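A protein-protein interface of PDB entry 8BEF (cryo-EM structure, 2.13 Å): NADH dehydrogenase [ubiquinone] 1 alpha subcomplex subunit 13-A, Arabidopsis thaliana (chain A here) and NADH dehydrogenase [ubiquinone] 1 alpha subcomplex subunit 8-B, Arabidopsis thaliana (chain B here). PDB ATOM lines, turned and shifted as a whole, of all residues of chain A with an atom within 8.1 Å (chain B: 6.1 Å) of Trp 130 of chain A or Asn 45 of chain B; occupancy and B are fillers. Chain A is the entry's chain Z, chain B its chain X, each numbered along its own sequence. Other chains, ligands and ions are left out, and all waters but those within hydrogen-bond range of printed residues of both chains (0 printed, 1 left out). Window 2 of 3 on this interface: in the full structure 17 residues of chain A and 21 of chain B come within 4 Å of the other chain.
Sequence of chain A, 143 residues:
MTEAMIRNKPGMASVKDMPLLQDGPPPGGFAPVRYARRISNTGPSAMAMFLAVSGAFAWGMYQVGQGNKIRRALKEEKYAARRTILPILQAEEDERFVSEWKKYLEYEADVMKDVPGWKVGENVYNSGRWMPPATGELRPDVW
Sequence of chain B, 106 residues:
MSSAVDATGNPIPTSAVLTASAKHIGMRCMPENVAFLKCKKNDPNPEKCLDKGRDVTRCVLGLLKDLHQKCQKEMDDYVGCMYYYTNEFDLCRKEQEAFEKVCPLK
OD2 of Asp 94 of chain A is in salt-bridge range of NZ of Lys 40 of chain B, at 2.9 Å.
The indole nitrogen of Trp 130 of chain A sits close to the side-chain amide oxygen of Asn 45 of chain B (3.4 Å).
CB of Pro 46 of chain B touches OD1 of Asp 94 of chain A (3.4 Å).
Phe 97 of chain A touches Pro 46 of chain B (CD2 to CG, 3.7 Å).
N of Glu 47 of chain B touches CG2 of Val 98 of chain A, 3.9 Å away.
Pro 44 of chain B touches Trp 130 of chain A (O to CZ3, 3.7 Å).
CD of Pro 46 of chain B touches CZ2 of Trp 130 of chain A (3.5 Å).
Of the printed residues of chain B, Trp 130 of chain A touches Pro 44 (3.7 Å), Asn 45 (3.4 Å) and Pro 46 (3.5 Å).
Asn 45 of chain B touches just one residue of chain A: Trp 130.
Of the printed residues of chain B, Phe 97 of chain A touches Pro 46.
Of the printed residues of chain A, Pro 46 of chain B touches Asp 94, Phe 97 and Trp 130.
Of the printed residues of chain B, Asp 94 of chain A touches Lys 40 (2.9 Å) and Pro 46 (3.4 Å).
Printed residues of chain B within 4 Å of Val 98 of chain A: Glu 47 (3.9 Å).
Printed residues of chain B that touch a printed residue of chain A: Lys 40, Pro 44, Asn 45, Pro 46 and Glu 47.
Hydrophobic or aromatic side chains of chain B that line the printed part of chain A: Pro 46.
Among the printed residues, Asp or Glu carboxylates within 4 Å of a Lys or Arg side-chain nitrogen of the other chain: Asp 94 of chain A with Lys 40 of chain B (2.9 Å).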
ATOM      1  N   ASP A  94     -33.651  17.022 -25.252  1.00  0.00           N
ATOM      2  CA  ASP A  94     -32.603  17.922 -25.720  1.00  0.00           C
ATOM      3  C   ASP A  94     -33.097  18.783 -26.875  1.00  0.00           C
ATOM      4  O   ASP A  94     -32.868  19.996 -26.901  1.00  0.00           O
ATOM      5  CB  ASP A  94     -31.371  17.119 -26.137  1.00  0.00           C
ATOM      6  CG  ASP A  94     -30.543  16.661 -24.952  1.00  0.00           C
ATOM      7  OD1 ASP A  94     -30.878  17.032 -23.809  1.00  0.00           O
ATOM      8  OD2 ASP A  94     -29.548  15.940 -25.169  1.00  0.00           O
ATOM      9  N   PHE A  97     -35.526  21.399 -25.461  1.00  0.00           N
ATOM     10  CA  PHE A  97     -34.852  22.469 -24.739  1.00  0.00           C
ATOM     11  C   PHE A  97     -34.091  23.386 -25.684  1.00  0.00           C
ATOM     12  O   PHE A  97     -34.040  24.597 -25.461  1.00  0.00           O
ATOM     13  CB  PHE A  97     -33.900  21.908 -23.687  1.00  0.00           C
ATOM     14  CG  PHE A  97     -33.154  22.973 -22.940  1.00  0.00           C
ATOM     15  CD1 PHE A  97     -33.730  23.605 -21.853  1.00  0.00           C
ATOM     16  CD2 PHE A  97     -31.893  23.372 -23.348  1.00  0.00           C
ATOM     17  CE1 PHE A  97     -33.054  24.597 -21.173  1.00  0.00           C
ATOM     18  CE2 PHE A  97     -31.216  24.368 -22.677  1.00  0.00           C
ATOM     19  CZ  PHE A  97     -31.796  24.977 -21.585  1.00  0.00           C
ATOM     20  N   VAL A  98     -33.463  22.830 -26.720  1.00  0.00           N
ATOM     21  CA  VAL A  98     -32.708  23.667 -27.645  1.00  0.00           C
ATOM     22  C   VAL A  98     -33.640  24.617 -28.386  1.00  0.00           C
ATOM     23  O   VAL A  98     -33.344  25.810 -28.530  1.00  0.00           O
ATOM     24  CB  VAL A  98     -31.884  22.797 -28.611  1.00  0.00           C
ATOM     25  CG1 VAL A  98     -31.365  23.631 -29.765  1.00  0.00           C
ATOM     26  CG2 VAL A  98     -30.728  22.156 -27.875  1.00  0.00           C
ATOM     27  N   TRP A 101     -34.731  27.294 -25.990  1.00  0.00           N
ATOM     28  CA  TRP A 101     -33.635  28.210 -25.703  1.00  0.00           C
ATOM     29  C   TRP A 101     -33.404  29.175 -26.857  1.00  0.00           C
ATOM     30  O   TRP A 101     -33.103  30.351 -26.632  1.00  0.00           O
ATOM     31  CB  TRP A 101     -32.359  27.428 -25.398  1.00  0.00           C
ATOM     32  CG  TRP A 101     -31.258  28.305 -24.915  1.00  0.00           C
ATOM     33  CD1 TRP A 101     -30.090  28.587 -25.559  1.00  0.00           C
ATOM     34  CD2 TRP A 101     -31.227  29.036 -23.688  1.00  0.00           C
ATOM     35  NE1 TRP A 101     -29.329  29.444 -24.804  1.00  0.00           N
ATOM     36  CE2 TRP A 101     -30.006  29.734 -23.649  1.00  0.00           C
ATOM     37  CE3 TRP A 101     -32.114  29.166 -22.613  1.00  0.00           C
ATOM     38  CZ2 TRP A 101     -29.649  30.548 -22.583  1.00  0.00           C
ATOM     39  CZ3 TRP A 101     -31.755  29.973 -21.553  1.00  0.00           C
ATOM     40  CH2 TRP A 101     -30.533  30.655 -21.547  1.00  0.00           C
ATOM     41  N   ASN A 123     -22.800  33.531 -20.927  1.00  0.00           N
ATOM     42  CA  ASN A 123     -22.574  32.551 -19.871  1.00  0.00           C
ATOM     43  C   ASN A 123     -21.976  33.242 -18.651  1.00  0.00           C
ATOM     44  O   ASN A 123     -20.923  33.879 -18.746  1.00  0.00           O
ATOM     45  CB  ASN A 123     -21.649  31.445 -20.371  1.00  0.00           C
ATOM     46  CG  ASN A 123     -21.669  30.211 -19.484  1.00  0.00           C
ATOM     47  OD1 ASN A 123     -22.047  30.271 -18.314  1.00  0.00           O
ATOM     48  ND2 ASN A 123     -21.252  29.084 -20.041  1.00  0.00           N
ATOM     49  N   TYR A 125     -20.784  31.738 -16.041  1.00  0.00           N
ATOM     50  CA  TYR A 125     -19.668  30.958 -15.525  1.00  0.00           C
ATOM     51  C   TYR A 125     -18.412  31.237 -16.341  1.00  0.00           C
ATOM     52  O   TYR A 125     -18.442  31.200 -17.575  1.00  0.00           O
ATOM     53  CB  TYR A 125     -20.006  29.468 -15.550  1.00  0.00           C
ATOM     54  CG  TYR A 125     -21.082  29.091 -14.558  1.00  0.00           C
ATOM     55  CD1 TYR A 125     -20.806  29.033 -13.199  1.00  0.00           C
ATOM     56  CD2 TYR A 125     -22.379  28.817 -14.977  1.00  0.00           C
ATOM     57  CE1 TYR A 125     -21.781  28.703 -12.285  1.00  0.00           C
ATOM     58  CE2 TYR A 125     -23.364  28.482 -14.068  1.00  0.00           C
ATOM     59  CZ  TYR A 125     -23.057  28.427 -12.721  1.00  0.00           C
ATOM     60  OH  TYR A 125     -24.024  28.098 -11.807  1.00  0.00           O
ATOM     61  N   SER A 127     -15.674  29.406 -16.514  1.00  0.00           N
ATOM     62  CA  SER A 127     -15.233  28.196 -17.193  1.00  0.00           C
ATOM     63  C   SER A 127     -15.981  27.960 -18.497  1.00  0.00           C
ATOM     64  O   SER A 127     -15.491  27.220 -19.355  1.00  0.00           O
ATOM     65  CB  SER A 127     -15.403  26.987 -16.274  1.00  0.00           C
ATOM     66  OG  SER A 127     -16.687  26.409 -16.426  1.00  0.00           O
ATOM     67  N   GLY A 128     -17.154  28.569 -18.665  1.00  0.00           N
ATOM     68  CA  GLY A 128     -17.945  28.393 -19.860  1.00  0.00           C
ATOM     69  C   GLY A 128     -18.629  27.052 -19.980  1.00  0.00           C
ATOM     70  O   GLY A 128     -19.325  26.818 -20.973  1.00  0.00           O
ATOM     71  N   ARG A 129     -18.463  26.167 -19.004  1.00  0.00           N
ATOM     72  CA  ARG A 129     -19.132  24.878 -19.061  1.00  0.00           C
ATOM     73  C   ARG A 129     -20.637  25.064 -18.902  1.00  0.00           C
ATOM     74  O   ARG A 129     -21.107  25.966 -18.203  1.00  0.00           O
ATOM     75  CB  ARG A 129     -18.559  23.935 -18.002  1.00  0.00           C
ATOM     76  CG  ARG A 129     -19.566  23.116 -17.227  1.00  0.00           C
ATOM     77  CD  ARG A 129     -18.849  22.171 -16.277  1.00  0.00           C
ATOM     78  NE  ARG A 129     -18.263  22.830 -15.116  1.00  0.00           N
ATOM     79  CZ  ARG A 129     -17.427  22.237 -14.271  1.00  0.00           C
ATOM     80  NH1 ARG A 129     -17.053  20.981 -14.439  1.00  0.00           N
ATOM     81  NH2 ARG A 129     -16.965  22.919 -13.229  1.00  0.00           N
ATOM     82  N   TRP A 130     -21.392  24.218 -19.590  1.00  0.00           N
ATOM     83  CA  TRP A 130     -22.830  24.403 -19.698  1.00  0.00           C
ATOM     84  C   TRP A 130     -23.529  23.962 -18.420  1.00  0.00           C
ATOM     85  O   TRP A 130     -23.254  22.884 -17.889  1.00  0.00           O
ATOM     86  CB  TRP A 130     -23.375  23.626 -20.892  1.00  0.00           C
ATOM     87  CG  TRP A 130     -24.810  23.909 -21.146  1.00  0.00           C
ATOM     88  CD1 TRP A 130     -25.324  24.944 -21.867  1.00  0.00           C
ATOM     89  CD2 TRP A 130     -25.928  23.158 -20.666  1.00  0.00           C
ATOM     90  NE1 TRP A 130     -26.694  24.881 -21.870  1.00  0.00           N
ATOM     91  CE2 TRP A 130     -27.090  23.791 -21.142  1.00  0.00           C
ATOM     92  CE3 TRP A 130     -26.057  22.005 -19.886  1.00  0.00           C
ATOM     93  CZ2 TRP A 130     -28.367  23.313 -20.862  1.00  0.00           C
ATOM     94  CZ3 TRP A 130     -27.324  21.532 -19.610  1.00  0.00           C
ATOM     95  CH2 TRP A 130     -28.462  22.186 -20.094  1.00  0.00           C
ATOM     96  N   MET A 131     -24.437  24.801 -17.935  1.00  0.00           N
ATOM     97  CA  MET A 131     -25.320  24.478 -16.828  1.00  0.00           C
ATOM     98  C   MET A 131     -26.753  24.789 -17.231  1.00  0.00           C
ATOM     99  O   MET A 131     -26.997  25.745 -17.973  1.00  0.00           O
ATOM    100  CB  MET A 131     -24.957  25.273 -15.564  1.00  0.00           C
ATOM    101  CG  MET A 131     -23.547  25.016 -15.040  1.00  0.00           C
ATOM    102  SD  MET A 131     -23.346  23.429 -14.207  1.00  0.00           S
ATOM    103  CE  MET A 131     -24.579  23.551 -12.914  1.00  0.00           C
ATOM    104  N   PRO A 132     -27.716  23.997 -16.767  1.00  0.00           N
ATOM    105  CA  PRO A 132     -29.112  24.317 -17.047  1.00  0.00           C
ATOM    106  C   PRO A 132     -29.493  25.630 -16.397  1.00  0.00           C
ATOM    107  O   PRO A 132     -28.903  26.032 -15.376  1.00  0.00           O
ATOM    108  CB  PRO A 132     -29.882  23.137 -16.429  1.00  0.00           C
ATOM    109  CG  PRO A 132     -28.877  22.118 -16.050  1.00  0.00           C
ATOM    110  CD  PRO A 132     -27.550  22.777 -15.961  1.00  0.00           C
ATOM    111  N   PRO A 133     -30.464  26.345 -16.961  1.00  0.00           N
ATOM    112  CA  PRO A 133     -30.878  27.617 -16.353  1.00  0.00           C
ATOM    113  C   PRO A 133     -31.445  27.398 -14.957  1.00  0.00           C
ATOM    114  O   PRO A 133     -32.264  26.503 -14.732  1.00  0.00           O
ATOM    115  CB  PRO A 133     -31.939  28.154 -17.323  1.00  0.00           C
ATOM    116  CG  PRO A 133     -31.854  27.295 -18.547  1.00  0.00           C
ATOM    117  CD  PRO A 133     -31.304  25.981 -18.112  1.00  0.00           C
ATOM    118  N   LYS B  40     -23.073  12.166 -24.079  1.00  0.00           N
ATOM    119  CA  LYS B  40     -23.670  12.855 -22.938  1.00  0.00           C
ATOM    120  C   LYS B  40     -22.719  12.878 -21.749  1.00  0.00           C
ATOM    121  O   LYS B  40     -22.638  13.880 -21.029  1.00  0.00           O
ATOM    122  CB  LYS B  40     -24.994  12.190 -22.552  1.00  0.00           C
ATOM    123  CG  LYS B  40     -26.165  12.535 -23.459  1.00  0.00           C
ATOM    124  CD  LYS B  40     -26.263  14.035 -23.686  1.00  0.00           C
ATOM    125  CE  LYS B  40     -26.866  14.745 -22.488  1.00  0.00           C
ATOM    126  NZ  LYS B  40     -27.810  15.819 -22.899  1.00  0.00           N
ATOM    127  N   ASP B  43     -20.206  15.582 -22.600  1.00  0.00           N
ATOM    128  CA  ASP B  43     -20.763  16.928 -22.658  1.00  0.00           C
ATOM    129  C   ASP B  43     -22.258  16.931 -22.365  1.00  0.00           C
ATOM    130  O   ASP B  43     -23.049  16.392 -23.149  1.00  0.00           O
ATOM    131  CB  ASP B  43     -20.496  17.552 -24.026  1.00  0.00           C
ATOM    132  CG  ASP B  43     -20.025  18.986 -23.928  1.00  0.00           C
ATOM    133  OD1 ASP B  43     -20.480  19.695 -23.010  1.00  0.00           O
ATOM    134  OD2 ASP B  43     -19.202  19.402 -24.769  1.00  0.00           O
ATOM    135  N   PRO B  44     -22.684  17.531 -21.251  1.00  0.00           N
ATOM    136  CA  PRO B  44     -24.120  17.611 -20.951  1.00  0.00           C
ATOM    137  C   PRO B  44     -24.870  18.665 -21.750  1.00  0.00           C
ATOM    138  O   PRO B  44     -26.105  18.708 -21.665  1.00  0.00           O
ATOM    139  CB  PRO B  44     -24.138  17.950 -19.456  1.00  0.00           C
ATOM    140  CG  PRO B  44     -22.878  18.720 -19.256  1.00  0.00           C
ATOM    141  CD  PRO B  44     -21.862  18.077 -20.157  1.00  0.00           C
ATOM    142  N   ASN B  45     -24.181  19.511 -22.505  1.00  0.00           N
ATOM    143  CA  ASN B  45     -24.856  20.541 -23.282  1.00  0.00           C
ATOM    144  C   ASN B  45     -25.721  19.880 -24.351  1.00  0.00           C
ATOM    145  O   ASN B  45     -25.192  19.143 -25.197  1.00  0.00           O
ATOM    146  CB  ASN B  45     -23.835  21.483 -23.917  1.00  0.00           C
ATOM    147  CG  ASN B  45     -24.475  22.700 -24.569  1.00  0.00           C
ATOM    148  OD1 ASN B  45     -25.687  22.897 -24.500  1.00  0.00           O
ATOM    149  ND2 ASN B  45     -23.656  23.529 -25.194  1.00  0.00           N
ATOM    150  N   PRO B  46     -27.039  20.095 -24.341  1.00  0.00           N
ATOM    151  CA  PRO B  46     -27.906  19.396 -25.304  1.00  0.00           C
ATOM    152  C   PRO B  46     -27.599  19.715 -26.755  1.00  0.00           C
ATOM    153  O   PRO B  46     -27.815  18.858 -27.621  1.00  0.00           O
ATOM    154  CB  PRO B  46     -29.315  19.867 -24.911  1.00  0.00           C
ATOM    155  CG  PRO B  46     -29.102  21.104 -24.094  1.00  0.00           C
ATOM    156  CD  PRO B  46     -27.812  20.898 -23.382  1.00  0.00           C
ATOM    157  N   GLU B  47     -27.115  20.922 -27.052  1.00  0.00           N
ATOM    158  CA  GLU B  47     -26.875  21.300 -28.442  1.00  0.00           C
ATOM    159  C   GLU B  47     -25.757  20.456 -29.043  1.00  0.00           C
ATOM    160  O   GLU B  47     -25.835  20.052 -30.209  1.00  0.00           O
ATOM    161  CB  GLU B  47     -26.581  22.808 -28.511  1.00  0.00           C
ATOM    162  CG  GLU B  47     -26.542  23.494 -29.899  1.00  0.00           C
ATOM    163  CD  GLU B  47     -25.622  22.860 -30.927  1.00  0.00           C
ATOM    164  OE1 GLU B  47     -25.998  22.823 -32.118  1.00  0.00           O
ATOM    165  OE2 GLU B  47     -24.490  22.474 -30.567  1.00  0.00           O
ATOM    166  N   LYS B  48     -24.737  20.137 -28.251  1.00  0.00           N
ATOM    167  CA  LYS B  48     -23.568  19.402 -28.714  1.00  0.00           C
ATOM    168  C   LYS B  48     -23.789  17.887 -28.777  1.00  0.00           C
ATOM    169  O   LYS B  48     -22.807  17.139 -28.788  1.00  0.00           O
ATOM    170  CB  LYS B  48     -22.371  19.713 -27.814  1.00  0.00           C
ATOM    171  CG  LYS B  48     -21.992  21.181 -27.787  1.00  0.00           C
ATOM    172  CD  LYS B  48     -20.492  21.360 -27.656  1.00  0.00           C
ATOM    173  CE  LYS B  48     -20.100  22.827 -27.704  1.00  0.00           C
ATOM    174  NZ  LYS B  48     -21.110  23.658 -28.415  1.00  0.00           N
ATOM    175  N   CYS B  49     -25.040  17.425 -28.810  1.00  0.00           N
ATOM    176  CA  CYS B  49     -25.334  15.996 -28.833  1.00  0.00           C
ATOM    177  C   CYS B  49     -26.489  15.659 -29.772  1.00  0.00           C
ATOM    178  O   CYS B  49     -26.927  14.502 -29.802  1.00  0.00           O
ATOM    179  CB  CYS B  49     -25.638  15.510 -27.406  1.00  0.00           C
ATOM    180  SG  CYS B  49     -25.783  13.725 -27.164  1.00  0.00           S
